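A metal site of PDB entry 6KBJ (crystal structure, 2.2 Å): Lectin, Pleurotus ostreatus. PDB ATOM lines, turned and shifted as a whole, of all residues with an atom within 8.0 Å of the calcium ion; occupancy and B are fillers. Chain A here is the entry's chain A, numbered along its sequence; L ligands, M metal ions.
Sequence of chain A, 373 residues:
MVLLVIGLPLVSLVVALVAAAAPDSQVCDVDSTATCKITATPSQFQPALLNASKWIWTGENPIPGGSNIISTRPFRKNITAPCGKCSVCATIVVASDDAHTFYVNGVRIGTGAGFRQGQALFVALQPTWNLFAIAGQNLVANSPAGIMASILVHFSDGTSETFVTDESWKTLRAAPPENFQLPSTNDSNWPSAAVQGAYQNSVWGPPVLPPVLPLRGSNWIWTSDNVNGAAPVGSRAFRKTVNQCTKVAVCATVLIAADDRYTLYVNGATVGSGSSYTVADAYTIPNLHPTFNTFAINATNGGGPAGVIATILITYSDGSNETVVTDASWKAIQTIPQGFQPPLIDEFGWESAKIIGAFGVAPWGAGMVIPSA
The backbone NH of Gly 302 sits close to the side-chain carboxylate of Asp 260, at 3.0 Å.
The backbone NH (N) of Asp 260 sits at hydrogen-bond distance from the backbone carbonyl oxygen (O) of Thr 300.
ND2 of Asn 301 lies within hydrogen-bond range of O of Gly 304.
The backbone carbonyl oxygen (O) of Ala 231 lies within hydrogen-bond range of the side-chain amide nitrogen (ND2) of Asn 301, 2.7 Å away.
The backbone carbonyl oxygen (O) of Pro 232 is in hydrogen-bond range of the side-chain amide nitrogen (ND2) of Asn 301 (3.0 Å).
The backbone carbonyl oxygen (O) of Val 233 sits close to the backbone carbonyl oxygen (O) of Asn 301, 2.7 Å away.
N of Asp 259 sits at hydrogen-bond distance from O of Gly 307, 2.8 Å away.
NE1 of Trp 364 is in hydrogen-bond range of OD2 of Asp 259, at 2.9 Å.
Merely in contact with the calcium ion: Gly 304.
Within 4 Å of the calcium ion: Asp 259, Asp 260, Asn 301, Gly 303, Gly 304 and Pro 305.
The calcium ion is bound by the backbone carbonyl oxygen of Pro 305, the side-chain carboxylate of Asp 260, the side-chain amide oxygen of Asn 301, an oxygen (O2) of the ligand, the side-chain carboxylate of Asp 259 and the backbone carbonyl oxygen of Gly 303.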
ATOM      1  N   TRP A 222     -27.772  24.194 -32.767  1.00  0.00           N
ATOM      2  CA  TRP A 222     -27.825  22.742 -32.827  1.00  0.00           C
ATOM      3  C   TRP A 222     -29.049  22.355 -33.672  1.00  0.00           C
ATOM      4  O   TRP A 222     -29.805  23.173 -34.232  1.00  0.00           O
ATOM      5  CB  TRP A 222     -27.919  22.146 -31.358  1.00  0.00           C
ATOM      6  CG  TRP A 222     -27.407  20.749 -31.087  1.00  0.00           C
ATOM      7  CD1 TRP A 222     -28.171  19.684 -30.787  1.00  0.00           C
ATOM      8  CD2 TRP A 222     -26.028  20.267 -31.095  1.00  0.00           C
ATOM      9  NE1 TRP A 222     -27.364  18.569 -30.632  1.00  0.00           N
ATOM     10  CE2 TRP A 222     -26.063  18.903 -30.818  1.00  0.00           C
ATOM     11  CE3 TRP A 222     -24.808  20.855 -31.364  1.00  0.00           C
ATOM     12  CZ2 TRP A 222     -24.943  18.133 -30.732  1.00  0.00           C
ATOM     13  CZ3 TRP A 222     -23.666  20.067 -31.287  1.00  0.00           C
ATOM     14  CH2 TRP A 222     -23.759  18.712 -30.953  1.00  0.00           C
ATOM     15  N   ASN A 226     -32.453  19.767 -29.249  1.00  0.00           N
ATOM     16  CA  ASN A 226     -31.901  20.455 -28.077  1.00  0.00           C
ATOM     17  C   ASN A 226     -33.068  21.285 -27.546  1.00  0.00           C
ATOM     18  O   ASN A 226     -33.475  22.246 -28.235  1.00  0.00           O
ATOM     19  CB  ASN A 226     -30.743  21.341 -28.565  1.00  0.00           C
ATOM     20  CG  ASN A 226     -29.894  21.886 -27.456  1.00  0.00           C
ATOM     21  OD1 ASN A 226     -30.413  22.368 -26.463  1.00  0.00           O
ATOM     22  ND2 ASN A 226     -28.570  21.888 -27.652  1.00  0.00           N
ATOM     23  N   GLY A 229     -32.498  23.064 -22.165  1.00  0.00           N
ATOM     24  CA  GLY A 229     -31.068  23.015 -21.778  1.00  0.00           C
ATOM     25  C   GLY A 229     -30.413  21.706 -22.141  1.00  0.00           C
ATOM     26  O   GLY A 229     -29.258  21.527 -21.692  1.00  0.00           O
ATOM     27  N   ALA A 230     -31.226  20.890 -22.891  1.00  0.00           N
ATOM     28  CA  ALA A 230     -31.129  19.542 -23.618  1.00  0.00           C
ATOM     29  C   ALA A 230     -29.869  18.871 -23.553  1.00  0.00           C
ATOM     30  O   ALA A 230     -29.447  18.784 -22.377  1.00  0.00           O
ATOM     31  CB  ALA A 230     -31.562  19.621 -25.061  1.00  0.00           C
ATOM     32  N   ALA A 231     -29.301  18.254 -24.638  1.00  0.00           N
ATOM     33  CA  ALA A 231     -29.879  17.498 -25.836  1.00  0.00           C
ATOM     34  C   ALA A 231     -29.370  16.064 -25.830  1.00  0.00           C
ATOM     35  O   ALA A 231     -28.408  15.771 -25.091  1.00  0.00           O
ATOM     36  CB  ALA A 231     -29.323  18.078 -27.177  1.00  0.00           C
ATOM     37  N   PRO A 232     -29.893  15.201 -26.736  1.00  0.00           N
ATOM     38  CA  PRO A 232     -29.463  13.791 -26.707  1.00  0.00           C
ATOM     39  C   PRO A 232     -27.996  13.587 -26.982  1.00  0.00           C
ATOM     40  O   PRO A 232     -27.301  14.473 -27.558  1.00  0.00           O
ATOM     41  CB  PRO A 232     -30.294  13.127 -27.835  1.00  0.00           C
ATOM     42  CG  PRO A 232     -31.491  13.997 -27.986  1.00  0.00           C
ATOM     43  CD  PRO A 232     -31.021  15.400 -27.675  1.00  0.00           C
ATOM     44  N   VAL A 233     -27.542  12.408 -26.628  1.00  0.00           N
ATOM     45  CA  VAL A 233     -26.183  11.986 -26.885  1.00  0.00           C
ATOM     46  C   VAL A 233     -25.702  11.762 -28.346  1.00  0.00           C
ATOM     47  O   VAL A 233     -24.537  11.660 -28.557  1.00  0.00           O
ATOM     48  CB  VAL A 233     -25.819  10.763 -26.026  1.00  0.00           C
ATOM     49  CG1 VAL A 233     -24.370  10.260 -26.214  1.00  0.00           C
ATOM     50  CG2 VAL A 233     -26.008  11.147 -24.557  1.00  0.00           C
ATOM     51  N   ALA A 258     -17.196  23.829 -29.874  1.00  0.00           N
ATOM     52  CA  ALA A 258     -18.404  23.118 -29.661  1.00  0.00           C
ATOM     53  C   ALA A 258     -18.485  22.436 -28.284  1.00  0.00           C
ATOM     54  O   ALA A 258     -17.523  21.914 -27.754  1.00  0.00           O
ATOM     55  CB  ALA A 258     -18.456  22.045 -30.734  1.00  0.00           C
ATOM     56  N   ASP A 259     -19.682  22.294 -27.827  1.00  0.00           N
ATOM     57  CA  ASP A 259     -19.931  21.417 -26.717  1.00  0.00           C
ATOM     58  C   ASP A 259     -20.556  20.096 -27.257  1.00  0.00           C
ATOM     59  O   ASP A 259     -21.744  20.104 -27.656  1.00  0.00           O
ATOM     60  CB  ASP A 259     -20.926  22.121 -25.813  1.00  0.00           C
ATOM     61  CG  ASP A 259     -21.268  21.317 -24.552  1.00  0.00           C
ATOM     62  OD1 ASP A 259     -20.823  20.136 -24.492  1.00  0.00           O
ATOM     63  OD2 ASP A 259     -21.940  21.882 -23.666  1.00  0.00           O
ATOM     64  N   ASP A 260     -19.902  18.945 -27.156  1.00  0.00           N
ATOM     65  CA  ASP A 260     -18.536  18.657 -26.617  1.00  0.00           C
ATOM     66  C   ASP A 260     -17.805  18.588 -27.864  1.00  0.00           C
ATOM     67  O   ASP A 260     -18.412  18.487 -28.920  1.00  0.00           O
ATOM     68  CB  ASP A 260     -18.666  17.276 -25.880  1.00  0.00           C
ATOM     69  CG  ASP A 260     -19.528  17.404 -24.585  1.00  0.00           C
ATOM     70  OD1 ASP A 260     -18.919  17.954 -23.677  1.00  0.00           O
ATOM     71  OD2 ASP A 260     -20.785  17.102 -24.464  1.00  0.00           O
ATOM     72  N   ARG A 261     -16.547  18.566 -27.987  1.00  0.00           N
ATOM     73  CA  ARG A 261     -16.213  18.184 -29.565  1.00  0.00           C
ATOM     74  C   ARG A 261     -16.837  18.434 -31.095  1.00  0.00           C
ATOM     75  O   ARG A 261     -18.037  18.464 -31.384  1.00  0.00           O
ATOM     76  CB  ARG A 261     -15.694  16.704 -29.588  1.00  0.00           C
ATOM     77  CG  ARG A 261     -16.662  15.557 -29.825  1.00  0.00           C
ATOM     78  CD  ARG A 261     -16.008  14.131 -29.719  1.00  0.00           C
ATOM     79  NE  ARG A 261     -14.557  14.112 -29.513  1.00  0.00           N
ATOM     80  CZ  ARG A 261     -13.936  13.976 -28.308  1.00  0.00           C
ATOM     81  NH1 ARG A 261     -14.644  13.817 -27.155  1.00  0.00           N
ATOM     82  NH2 ARG A 261     -12.595  14.038 -28.250  1.00  0.00           N
ATOM     83  N   TYR A 277     -15.316  23.413 -25.272  1.00  0.00           N
ATOM     84  CA  TYR A 277     -16.227  24.503 -25.291  1.00  0.00           C
ATOM     85  C   TYR A 277     -15.780  25.732 -24.472  1.00  0.00           C
ATOM     86  O   TYR A 277     -16.571  26.687 -24.387  1.00  0.00           O
ATOM     87  CB  TYR A 277     -17.627  24.070 -24.889  1.00  0.00           C
ATOM     88  CG  TYR A 277     -17.792  23.432 -23.551  1.00  0.00           C
ATOM     89  CD1 TYR A 277     -17.968  24.209 -22.440  1.00  0.00           C
ATOM     90  CD2 TYR A 277     -17.848  22.029 -23.409  1.00  0.00           C
ATOM     91  CE1 TYR A 277     -18.181  23.634 -21.187  1.00  0.00           C
ATOM     92  CE2 TYR A 277     -17.995  21.419 -22.181  1.00  0.00           C
ATOM     93  CZ  TYR A 277     -18.173  22.245 -21.063  1.00  0.00           C
ATOM     94  OH  TYR A 277     -18.415  21.753 -19.826  1.00  0.00           O
ATOM     95  N   THR A 300     -20.392  16.519 -31.844  1.00  0.00           N
ATOM     96  CA  THR A 300     -20.888  15.466 -31.009  1.00  0.00           C
ATOM     97  C   THR A 300     -21.226  15.928 -29.554  1.00  0.00           C
ATOM     98  O   THR A 300     -20.425  16.547 -28.901  1.00  0.00           O
ATOM     99  CB  THR A 300     -19.835  14.348 -30.975  1.00  0.00           C
ATOM    100  OG1 THR A 300     -19.494  13.910 -32.332  1.00  0.00           O
ATOM    101  CG2 THR A 300     -20.336  13.180 -30.123  1.00  0.00           C
ATOM    102  N   ASN A 301     -22.412  15.579 -29.066  1.00  0.00           N
ATOM    103  CA  ASN A 301     -22.775  15.729 -27.685  1.00  0.00           C
ATOM    104  C   ASN A 301     -22.472  14.450 -26.872  1.00  0.00           C
ATOM    105  O   ASN A 301     -22.986  13.385 -27.151  1.00  0.00           O
ATOM    106  CB  ASN A 301     -24.228  16.160 -27.559  1.00  0.00           C
ATOM    107  CG  ASN A 301     -24.585  16.498 -26.090  1.00  0.00           C
ATOM    108  OD1 ASN A 301     -23.673  16.747 -25.328  1.00  0.00           O
ATOM    109  ND2 ASN A 301     -25.844  16.394 -25.693  1.00  0.00           N
ATOM    110  N   GLY A 302     -21.564  14.555 -25.905  1.00  0.00           N
ATOM    111  CA  GLY A 302     -21.279  13.494 -24.936  1.00  0.00           C
ATOM    112  C   GLY A 302     -22.312  13.359 -23.805  1.00  0.00           C
ATOM    113  O   GLY A 302     -22.318  12.386 -23.061  1.00  0.00           O
ATOM    114  N   GLY A 303     -23.184  14.346 -23.682  1.00  0.00           N
ATOM    115  CA  GLY A 303     -24.296  14.354 -22.759  1.00  0.00           C
ATOM    116  C   GLY A 303     -24.397  15.744 -22.163  1.00  0.00           C
ATOM    117  O   GLY A 303     -23.372  16.406 -21.989  1.00  0.00           O
ATOM    118  N   GLY A 304     -25.629  16.155 -21.874  1.00  0.00           N
ATOM    119  CA  GLY A 304     -25.910  17.430 -21.289  1.00  0.00           C
ATOM    120  C   GLY A 304     -26.297  18.451 -22.347  1.00  0.00           C
ATOM    121  O   GLY A 304     -26.827  18.087 -23.386  1.00  0.00           O
ATOM    122  N   PRO A 305     -26.064  19.760 -22.060  1.00  0.00           N
ATOM    123  CA  PRO A 305     -26.306  20.836 -23.054  1.00  0.00           C
ATOM    124  C   PRO A 305     -25.411  20.589 -24.231  1.00  0.00           C
ATOM    125  O   PRO A 305     -24.358  19.901 -24.098  1.00  0.00           O
ATOM    126  CB  PRO A 305     -25.843  22.119 -22.311  1.00  0.00           C
ATOM    127  CG  PRO A 305     -25.985  21.787 -20.858  1.00  0.00           C
ATOM    128  CD  PRO A 305     -25.512  20.334 -20.806  1.00  0.00           C
ATOM    129  N   ALA A 306     -25.775  21.141 -25.387  1.00  0.00           N
ATOM    130  CA  ALA A 306     -24.882  20.973 -26.551  1.00  0.00           C
ATOM    131  C   ALA A 306     -24.973  22.130 -27.455  1.00  0.00           C
ATOM    132  O   ALA A 306     -26.015  22.815 -27.502  1.00  0.00           O
ATOM    133  CB  ALA A 306     -25.245  19.695 -27.304  1.00  0.00           C
ATOM    134  N   GLY A 307     -23.928  22.341 -28.243  1.00  0.00           N
ATOM    135  CA  GLY A 307     -23.995  23.490 -29.212  1.00  0.00           C
ATOM    136  C   GLY A 307     -22.761  23.560 -30.031  1.00  0.00           C
ATOM    137  O   GLY A 307     -21.676  23.078 -29.598  1.00  0.00           O
ATOM    138  N   TRP A 364     -22.666  28.457 -21.225  1.00  0.00           N
ATOM    139  CA  TRP A 364     -21.239  28.578 -21.570  1.00  0.00           C
ATOM    140  C   TRP A 364     -20.722  29.972 -21.195  1.00  0.00           C
ATOM    141  O   TRP A 364     -19.544  30.119 -20.999  1.00  0.00           O
ATOM    142  CB  TRP A 364     -21.052  28.348 -23.114  1.00  0.00           C
ATOM    143  CG  TRP A 364     -21.711  27.014 -23.514  1.00  0.00           C
ATOM    144  CD1 TRP A 364     -21.194  25.778 -23.296  1.00  0.00           C
ATOM    145  CD2 TRP A 364     -22.945  26.818 -24.228  1.00  0.00           C
ATOM    146  NE1 TRP A 364     -22.079  24.823 -23.763  1.00  0.00           N
ATOM    147  CE2 TRP A 364     -23.140  25.441 -24.338  1.00  0.00           C
ATOM    148  CE3 TRP A 364     -23.899  27.668 -24.775  1.00  0.00           C
ATOM    149  CZ2 TRP A 364     -24.242  24.898 -24.947  1.00  0.00           C
ATOM    150  CZ3 TRP A 364     -25.017  27.129 -25.355  1.00  0.00           C
ATOM    151  CH2 TRP A 364     -25.185  25.751 -25.450  1.00  0.00           C
HETATM  152  C1  LIG L   1     -21.761  20.389 -21.179  1.00  0.00           C
HETATM  153  C2  LIG L   1     -20.957  18.956 -20.940  1.00  0.00           C
HETATM  154  C3  LIG L   1     -21.883  21.250 -19.889  1.00  0.00           C
HETATM  155  O1  LIG L   1     -20.378  18.672 -19.826  1.00  0.00           O
HETATM  156  O2  LIG L   1     -20.869  18.157 -21.929  1.00  0.00           O
HETATM  157  O3  LIG L   1     -21.501  20.683 -18.821  1.00  0.00           O
HETATM  158  O4  LIG L   1     -22.279  22.476 -19.960  1.00  0.00           O
HETATM  159 CA    CA M   1     -22.695  18.400 -23.711  1.00  0.00          CA
